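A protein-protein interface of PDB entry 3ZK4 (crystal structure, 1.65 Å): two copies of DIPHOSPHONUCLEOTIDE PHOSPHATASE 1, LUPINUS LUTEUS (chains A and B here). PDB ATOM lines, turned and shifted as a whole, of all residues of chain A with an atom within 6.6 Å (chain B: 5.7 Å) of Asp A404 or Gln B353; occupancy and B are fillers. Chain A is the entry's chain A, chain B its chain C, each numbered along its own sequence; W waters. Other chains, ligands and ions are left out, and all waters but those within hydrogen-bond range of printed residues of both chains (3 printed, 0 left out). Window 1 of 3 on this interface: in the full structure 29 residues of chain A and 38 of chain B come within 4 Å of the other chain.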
ATOM      1  N   ARG A 376       7.991  -2.964  23.240  1.00  0.00           N
ATOM      2  CA  ARG A 376       7.938  -4.434  23.133  1.00  0.00           C
ATOM      3  C   ARG A 376       8.068  -4.971  24.548  1.00  0.00           C
ATOM      4  O   ARG A 376       8.957  -4.547  25.331  1.00  0.00           O
ATOM      5  CB  ARG A 376       9.050  -4.969  22.228  1.00  0.00           C
ATOM      6  CG  ARG A 376       9.370  -6.457  22.433  1.00  0.00           C
ATOM      7  CD  ARG A 376       8.247  -7.321  21.873  1.00  0.00           C
ATOM      8  NE  ARG A 376       8.195  -7.285  20.422  1.00  0.00           N
ATOM      9  CZ  ARG A 376       8.941  -8.032  19.609  1.00  0.00           C
ATOM     10  NH1 ARG A 376       9.824  -8.907  20.102  1.00  0.00           N
ATOM     11  NH2 ARG A 376       8.802  -7.898  18.304  1.00  0.00           N
ATOM     12  N   ALA A 401      15.364 -10.534  20.547  1.00  0.00           N
ATOM     13  CA  ALA A 401      16.132 -10.327  19.315  1.00  0.00           C
ATOM     14  C   ALA A 401      15.290  -9.828  18.147  1.00  0.00           C
ATOM     15  O   ALA A 401      15.818  -9.215  17.219  1.00  0.00           O
ATOM     16  CB  ALA A 401      16.839 -11.631  18.921  1.00  0.00           C
ATOM     17  N   SER A 402      13.977 -10.073  18.173  1.00  0.00           N
ATOM     18  CA  SER A 402      13.124  -9.861  17.033  1.00  0.00           C
ATOM     19  C   SER A 402      12.598  -8.443  16.955  1.00  0.00           C
ATOM     20  O   SER A 402      11.972  -8.109  15.975  1.00  0.00           O
ATOM     21  CB  SER A 402      11.916 -10.830  17.008  1.00  0.00           C
ATOM     22  OG  SER A 402      11.031 -10.574  18.095  1.00  0.00           O
ATOM     23  N   VAL A 403      12.861  -7.619  17.951  1.00  0.00           N
ATOM     24  CA  VAL A 403      12.376  -6.244  17.932  1.00  0.00           C
ATOM     25  C   VAL A 403      13.299  -5.282  17.154  1.00  0.00           C
ATOM     26  O   VAL A 403      14.519  -5.266  17.370  1.00  0.00           O
ATOM     27  CB  VAL A 403      12.082  -5.729  19.377  1.00  0.00           C
ATOM     28  CG1 VAL A 403      13.299  -5.696  20.241  1.00  0.00           C
ATOM     29  CG2 VAL A 403      11.443  -4.355  19.330  1.00  0.00           C
ATOM     30  N   ASP A 404      12.676  -4.440  16.316  1.00  0.00           N
ATOM     31  CA  ASP A 404      13.358  -3.337  15.570  1.00  0.00           C
ATOM     32  C   ASP A 404      13.402  -2.147  16.523  1.00  0.00           C
ATOM     33  O   ASP A 404      12.366  -1.563  16.785  1.00  0.00           O
ATOM     34  CB  ASP A 404      12.527  -3.016  14.337  1.00  0.00           C
ATOM     35  CG  ASP A 404      13.060  -1.835  13.500  1.00  0.00           C
ATOM     36  OD1 ASP A 404      13.775  -0.942  14.044  1.00  0.00           O
ATOM     37  OD2 ASP A 404      12.674  -1.828  12.316  1.00  0.00           O
ATOM     38  N   ARG A 405      14.556  -1.832  17.079  1.00  0.00           N
ATOM     39  CA  ARG A 405      14.672  -0.885  18.185  1.00  0.00           C
ATOM     40  C   ARG A 405      14.638   0.575  17.704  1.00  0.00           C
ATOM     41  O   ARG A 405      14.519   1.509  18.525  1.00  0.00           O
ATOM     42  CB  ARG A 405      15.938  -1.129  18.970  1.00  0.00           C
ATOM     43  CG  ARG A 405      15.934  -2.380  19.822  1.00  0.00           C
ATOM     44  CD  ARG A 405      14.873  -2.375  20.904  1.00  0.00           C
ATOM     45  NE  ARG A 405      15.175  -1.590  22.094  1.00  0.00           N
ATOM     46  CZ  ARG A 405      16.063  -1.889  23.022  1.00  0.00           C
ATOM     47  NH1 ARG A 405      16.845  -2.970  22.922  1.00  0.00           N
ATOM     48  NH2 ARG A 405      16.178  -1.104  24.071  1.00  0.00           N
ATOM     49  N   GLN A 406      14.701   0.766  16.405  1.00  0.00           N
ATOM     50  CA  GLN A 406      14.475   2.115  15.869  1.00  0.00           C
ATOM     51  C   GLN A 406      12.985   2.456  15.953  1.00  0.00           C
ATOM     52  O   GLN A 406      12.619   3.526  16.441  1.00  0.00           O
ATOM     53  CB  GLN A 406      14.969   2.232  14.444  1.00  0.00           C
ATOM     54  CG  GLN A 406      14.678   3.596  13.806  1.00  0.00           C
ATOM     55  CD  GLN A 406      13.535   3.533  12.848  1.00  0.00           C
ATOM     56  OE1 GLN A 406      13.474   2.679  11.947  1.00  0.00           O
ATOM     57  NE2 GLN A 406      12.594   4.442  13.041  1.00  0.00           N
ATOM     58  N   LYS A 407      12.158   1.532  15.541  1.00  0.00           N
ATOM     59  CA  LYS A 407      10.702   1.697  15.549  1.00  0.00           C
ATOM     60  C   LYS A 407      10.154   1.529  16.963  1.00  0.00           C
ATOM     61  O   LYS A 407       9.265   2.253  17.391  1.00  0.00           O
ATOM     62  CB  LYS A 407      10.055   0.720  14.562  1.00  0.00           C
ATOM     63  CG  LYS A 407      10.375   1.024  13.084  1.00  0.00           C
ATOM     64  CD  LYS A 407       9.809  -0.028  12.144  1.00  0.00           C
ATOM     65  CE  LYS A 407      10.304   0.103  10.681  1.00  0.00           C
ATOM     66  NZ  LYS A 407      11.783   0.288  10.552  1.00  0.00           N
ATOM     67  N   GLN A 408      10.699   0.564  17.697  1.00  0.00           N
ATOM     68  CA  GLN A 408      10.201   0.203  19.028  1.00  0.00           C
ATOM     69  C   GLN A 408      11.339   0.292  20.021  1.00  0.00           C
ATOM     70  O   GLN A 408      11.992  -0.721  20.413  1.00  0.00           O
ATOM     71  CB  GLN A 408       9.620  -1.207  19.027  1.00  0.00           C
ATOM     72  CG  GLN A 408       8.374  -1.351  18.202  1.00  0.00           C
ATOM     73  CD  GLN A 408       7.752  -2.711  18.402  1.00  0.00           C
ATOM     74  OE1 GLN A 408       8.094  -3.650  17.695  1.00  0.00           O
ATOM     75  NE2 GLN A 408       6.826  -2.820  19.362  1.00  0.00           N
ATOM     76  N   PRO A 409      11.653   1.500  20.444  1.00  0.00           N
ATOM     77  CA  PRO A 409      12.832   1.617  21.301  1.00  0.00           C
ATOM     78  C   PRO A 409      12.755   0.989  22.671  1.00  0.00           C
ATOM     79  O   PRO A 409      13.781   0.676  23.215  1.00  0.00           O
ATOM     80  CB  PRO A 409      12.997   3.126  21.478  1.00  0.00           C
ATOM     81  CG  PRO A 409      11.728   3.715  21.071  1.00  0.00           C
ATOM     82  CD  PRO A 409      11.093   2.821  20.079  1.00  0.00           C
ATOM     83  N   TYR A 553      18.276   6.310  18.938  1.00  0.00           N
ATOM     84  CA  TYR A 553      18.559   4.998  18.328  1.00  0.00           C
ATOM     85  C   TYR A 553      20.059   4.681  18.365  1.00  0.00           C
ATOM     86  O   TYR A 553      20.470   3.587  18.736  1.00  0.00           O
ATOM     87  CB  TYR A 553      18.005   5.000  16.937  1.00  0.00           C
ATOM     88  CG  TYR A 553      18.208   3.747  16.150  1.00  0.00           C
ATOM     89  CD1 TYR A 553      17.953   2.465  16.712  1.00  0.00           C
ATOM     90  CD2 TYR A 553      18.592   3.804  14.806  1.00  0.00           C
ATOM     91  CE1 TYR A 553      18.105   1.320  15.952  1.00  0.00           C
ATOM     92  CE2 TYR A 553      18.742   2.652  14.038  1.00  0.00           C
ATOM     93  CZ  TYR A 553      18.521   1.419  14.624  1.00  0.00           C
ATOM     94  OH  TYR A 553      18.620   0.299  13.860  1.00  0.00           O
ATOM     95  N   CYS B 348      22.476   5.266   9.067  1.00  0.00           N
ATOM     96  CA  CYS B 348      22.447   4.006   9.844  1.00  0.00           C
ATOM     97  C   CYS B 348      21.186   3.177   9.642  1.00  0.00           C
ATOM     98  O   CYS B 348      20.629   2.609  10.609  1.00  0.00           O
ATOM     99  CB  CYS B 348      22.774   4.245  11.299  1.00  0.00           C
ATOM    100  SG  CYS B 348      21.699   5.394  12.256  1.00  0.00           S
ATOM    101  N   GLY B 349      20.783   3.065   8.396  1.00  0.00           N
ATOM    102  CA  GLY B 349      19.696   2.232   7.938  1.00  0.00           C
ATOM    103  C   GLY B 349      18.293   2.807   8.091  1.00  0.00           C
ATOM    104  O   GLY B 349      17.356   2.242   7.567  1.00  0.00           O
ATOM    105  N   VAL B 350      18.154   3.907   8.809  1.00  0.00           N
ATOM    106  CA  VAL B 350      16.808   4.387   9.194  1.00  0.00           C
ATOM    107  C   VAL B 350      15.929   4.762   8.028  1.00  0.00           C
ATOM    108  O   VAL B 350      14.795   4.245   7.882  1.00  0.00           O
ATOM    109  CB  VAL B 350      16.918   5.468  10.272  1.00  0.00           C
ATOM    110  CG1 VAL B 350      15.540   6.024  10.615  1.00  0.00           C
ATOM    111  CG2 VAL B 350      17.566   4.889  11.538  1.00  0.00           C
ATOM    112  N   PRO B 351      16.410   5.640   7.120  1.00  0.00           N
ATOM    113  CA  PRO B 351      15.561   5.889   5.954  1.00  0.00           C
ATOM    114  C   PRO B 351      15.212   4.644   5.144  1.00  0.00           C
ATOM    115  O   PRO B 351      14.067   4.438   4.742  1.00  0.00           O
ATOM    116  CB  PRO B 351      16.394   6.917   5.133  1.00  0.00           C
ATOM    117  CG  PRO B 351      17.268   7.553   6.135  1.00  0.00           C
ATOM    118  CD  PRO B 351      17.651   6.408   7.078  1.00  0.00           C
ATOM    119  N   ALA B 352      16.179   3.778   4.880  1.00  0.00           N
ATOM    120  CA  ALA B 352      15.900   2.636   4.051  1.00  0.00           C
ATOM    121  C   ALA B 352      14.823   1.706   4.643  1.00  0.00           C
ATOM    122  O   ALA B 352      13.991   1.167   3.909  1.00  0.00           O
ATOM    123  CB  ALA B 352      17.150   1.820   3.833  1.00  0.00           C
ATOM    124  N   GLN B 353      14.909   1.534   5.959  1.00  0.00           N
ATOM    125  CA  GLN B 353      14.014   0.614   6.675  1.00  0.00           C
ATOM    126  C   GLN B 353      12.661   1.245   7.004  1.00  0.00           C
ATOM    127  O   GLN B 353      11.809   0.567   7.557  1.00  0.00           O
ATOM    128  CB  GLN B 353      14.650   0.027   7.953  1.00  0.00           C
ATOM    129  CG  GLN B 353      14.916   1.011   9.092  1.00  0.00           C
ATOM    130  CD  GLN B 353      15.424   0.382  10.399  1.00  0.00           C
ATOM    131  OE1 GLN B 353      16.604   0.086  10.543  1.00  0.00           O
ATOM    132  NE2 GLN B 353      14.544   0.232  11.357  1.00  0.00           N
ATOM    133  N   THR B 354      12.475   2.525   6.642  1.00  0.00           N
ATOM    134  CA  THR B 354      11.200   3.237   6.831  1.00  0.00           C
ATOM    135  C   THR B 354      10.544   3.564   5.499  1.00  0.00           C
ATOM    136  O   THR B 354       9.349   3.330   5.307  1.00  0.00           O
ATOM    137  CB  THR B 354      11.413   4.507   7.649  1.00  0.00           C
ATOM    138  OG1 THR B 354      12.084   4.188   8.874  1.00  0.00           O
ATOM    139  CG2 THR B 354      10.085   5.199   7.921  1.00  0.00           C
ATOM    140  N   MET B 355      11.328   4.028   4.527  1.00  0.00           N
ATOM    141  CA  MET B 355      10.775   4.422   3.223  1.00  0.00           C
ATOM    142  C   MET B 355      10.232   3.235   2.443  1.00  0.00           C
ATOM    143  O   MET B 355       9.312   3.365   1.662  1.00  0.00           O
ATOM    144  CB  MET B 355      11.853   5.160   2.369  1.00  0.00           C
ATOM    145  CG  MET B 355      12.486   6.353   3.058  1.00  0.00           C
ATOM    146  SD  MET B 355      11.299   7.706   3.391  1.00  0.00           S
ATOM    147  CE  MET B 355      10.641   8.026   1.764  1.00  0.00           C
ATOM    148  N   PHE B 356      10.832   2.049   2.673  1.00  0.00           N
ATOM    149  CA  PHE B 356      10.478   0.852   1.984  1.00  0.00           C
ATOM    150  C   PHE B 356      10.079  -0.235   2.993  1.00  0.00           C
ATOM    151  O   PHE B 356      10.617  -0.275   4.100  1.00  0.00           O
ATOM    152  CB  PHE B 356      11.678   0.367   1.160  1.00  0.00           C
ATOM    153  CG  PHE B 356      11.910   1.223  -0.053  1.00  0.00           C
ATOM    154  CD1 PHE B 356      11.136   1.039  -1.166  1.00  0.00           C
ATOM    155  CD2 PHE B 356      12.806   2.240  -0.005  1.00  0.00           C
ATOM    156  CE1 PHE B 356      11.281   1.850  -2.285  1.00  0.00           C
ATOM    157  CE2 PHE B 356      12.948   3.092  -1.107  1.00  0.00           C
ATOM    158  CZ  PHE B 356      12.192   2.863  -2.226  1.00  0.00           C
ATOM    159  N   ASN B 362      12.128  -8.702  11.346  1.00  0.00           N
ATOM    160  CA  ASN B 362      12.700  -7.546  11.997  1.00  0.00           C
ATOM    161  C   ASN B 362      13.253  -6.629  10.884  1.00  0.00           C
ATOM    162  O   ASN B 362      14.248  -6.933  10.236  1.00  0.00           O
ATOM    163  CB  ASN B 362      13.786  -7.977  12.968  1.00  0.00           C
ATOM    164  CG  ASN B 362      14.394  -6.838  13.744  1.00  0.00           C
ATOM    165  OD1 ASN B 362      14.372  -5.702  13.279  1.00  0.00           O
ATOM    166  ND2 ASN B 362      15.044  -7.141  14.884  1.00  0.00           N
ATOM    167  N   ARG B 363      12.561  -5.505  10.636  1.00  0.00           N
ATOM    168  CA  ARG B 363      12.962  -4.657   9.503  1.00  0.00           C
ATOM    169  C   ARG B 363      14.322  -4.019   9.685  1.00  0.00           C
ATOM    170  O   ARG B 363      14.962  -3.629   8.707  1.00  0.00           O
ATOM    171  CB  ARG B 363      11.875  -3.603   9.265  1.00  0.00           C
ATOM    172  CG  ARG B 363      10.647  -4.228   8.588  1.00  0.00           C
ATOM    173  CD  ARG B 363       9.443  -3.286   8.632  1.00  0.00           C
ATOM    174  NE  ARG B 363       9.582  -2.181   7.671  1.00  0.00           N
ATOM    175  CZ  ARG B 363       8.700  -1.202   7.542  1.00  0.00           C
ATOM    176  NH1 ARG B 363       7.636  -1.142   8.370  1.00  0.00           N
ATOM    177  NH2 ARG B 363       8.869  -0.279   6.609  1.00  0.00           N
ATOM    178  N   GLU B 364      14.809  -3.951  10.919  1.00  0.00           N
ATOM    179  CA  GLU B 364      16.173  -3.496  11.178  1.00  0.00           C
ATOM    180  C   GLU B 364      17.197  -4.488  10.627  1.00  0.00           C
ATOM    181  O   GLU B 364      18.210  -4.083  10.041  1.00  0.00           O
ATOM    182  CB  GLU B 364      16.321  -3.263  12.673  1.00  0.00           C
ATOM    183  CG  GLU B 364      17.663  -2.862  13.135  1.00  0.00           C
ATOM    184  CD  GLU B 364      17.745  -2.692  14.667  1.00  0.00           C
ATOM    185  OE1 GLU B 364      16.773  -2.919  15.453  1.00  0.00           O
ATOM    186  OE2 GLU B 364      18.870  -2.416  15.089  1.00  0.00           O
ATOM    187  N   PHE B 366      16.628  -6.727   8.039  1.00  0.00           N
ATOM    188  CA  PHE B 366      16.507  -6.536   6.591  1.00  0.00           C
ATOM    189  C   PHE B 366      16.856  -7.809   5.802  1.00  0.00           C
ATOM    190  O   PHE B 366      17.218  -7.723   4.638  1.00  0.00           O
ATOM    191  CB  PHE B 366      17.411  -5.329   6.149  1.00  0.00           C
ATOM    192  CG  PHE B 366      16.768  -4.375   5.171  1.00  0.00           C
ATOM    193  CD1 PHE B 366      16.216  -4.821   3.992  1.00  0.00           C
ATOM    194  CD2 PHE B 366      16.799  -3.010   5.431  1.00  0.00           C
ATOM    195  CE1 PHE B 366      15.643  -3.923   3.086  1.00  0.00           C
ATOM    196  CE2 PHE B 366      16.235  -2.101   4.535  1.00  0.00           C
ATOM    197  CZ  PHE B 366      15.677  -2.561   3.384  1.00  0.00           C
HETATM  198  O   HOH W   1      19.135   0.468  11.353  1.00  0.00           O
HETATM  199  O   HOH W   2      10.072   4.404  11.568  1.00  0.00           O
HETATM  200  O   HOH W   3      17.213  -5.501  16.308  1.00  0.00           O
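Val A403 touches Glu B364 (O to OE1, 3.8 Å).
Asn B362 touches Asp A404 (OD1 to CB, 3.4 Å).
Asp A404 touches Arg B363.
Gln A406 touches Val B350.
Gln A406 touches Thr B354 (OE1 to OG1, 3.7 Å).
Arg B363 touches Lys A407.
Tyr A553 touches Cys B348.
Tyr A553 touches Val B350.
OE1 of Gln B353 touches OH of Tyr A553 (3.9 Å).
Hydrophobic or aromatic side chains of chain B that line the printed part of chain A: Val B350.
Of the 11 printed residues of chain A, 8 touch a printed residue of chain B.
Printed residues of chain A that touch a printed residue of chain B: Ala A401, Ser A402, Val A403, Asp A404, Arg A405, Gln A406, Lys A407 and Tyr A553.
Along chain A the printed residues that touch a printed residue of chain B span positions 401 to 553.
Of the printed residues of chain B, Asp A404 touches Gln B353, Asn B362, Arg B363 and Glu B364.
Printed residues of chain A within 4 Å of Gln B353: Asp A404, Gln A406, Lys A407 and Tyr A553.
Printed residues of chain A within 4 Å of Glu B364: Val A403, Asp A404, Arg A405 and Tyr A553.
Printed residues of chain B within 4 Å of Tyr A553: Cys B348, Val B350, Gln B353 and Glu B364.
Arg A376 touches none of the printed residues of chain B.
The nearest printed residue of chain B that does not touch Asp A404 is Thr B354 (7.0 Å).
The nearest printed residue of chain A that does not touch Thr B354 is Lys A407 (4.3 Å).
Water W1 lies within hydrogen-bond range of the side-chain hydroxyl of Tyr A553 (2.6 Å), the side-chain amide oxygen of Gln B353 (2.7 Å) and the backbone carbonyl oxygen of Cys B348 (2.7 Å).
Water W3 lies within hydrogen-bond range of OE1 of Glu B364 (2.8 Å), O of Val A403 (2.9 Å) and ND2 of Asn B362 (3.1 Å).
Water W2 lies within hydrogen-bond range of NE2 of Gln A406 (2.9 Å) and OG1 of Thr B354 (3.4 Å).
No position is printed for both chains.
O of Val A403 sits at hydrogen-bond distance from ND2 of Asn B362, 3.2 Å away.
The backbone NH of Glu B364 is in hydrogen-bond range of the side-chain carboxylate of Asp A404, at 3.3 Å.
OE1 of Gln A406 sits at hydrogen-bond distance from NE2 of Gln B353 (2.7 Å).
The side-chain carboxylate (OD2) of Asp A404 lies within hydrogen-bond range of the side-chain amide nitrogen (NE2) of Gln B353, 2.9 Å away.
The side-chain carboxylate of Glu B364 lies within hydrogen-bond range of the backbone NH of Arg A405.
The backbone carbonyl oxygen (O) of Ala A401 is in hydrogen-bond range of the side-chain amide nitrogen (ND2) of Asn B362 (3.2 Å).
The side-chain carboxylate (OE2) of Glu B364 lies within hydrogen-bond range of the side-chain hydroxyl (OH) of Tyr A553 (3.0 Å).
O of Ser A402 sits at hydrogen-bond distance from ND2 of Asn B362, 3.4 Å away.
The side-chain amino group (NZ) of Lys A407 lies close to the side-chain amide nitrogen (NE2) of Gln B353 (2.9 Å).
The side-chain hydroxyl (OG1) of Thr B354 sits at hydrogen-bond distance from the backbone carbonyl oxygen (O) of Val B350 (2.9 Å).
The backbone carbonyl oxygen (O) of Phe B356 is in hydrogen-bond range of the guanidinium group (NH2) of Arg B363, 3.1 Å away.
The backbone NH of Gln A406 lies within hydrogen-bond range of the side-chain carboxylate of Asp A404.
O of Pro A409 lies within hydrogen-bond range of NE of Arg A405 (2.9 Å).
NH1 of Arg A376 sits at hydrogen-bond distance from OG of Ser A402 (2.9 Å).
OD1 of Asn B362 lies within hydrogen-bond range of N of Glu B364 (3.0 Å).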
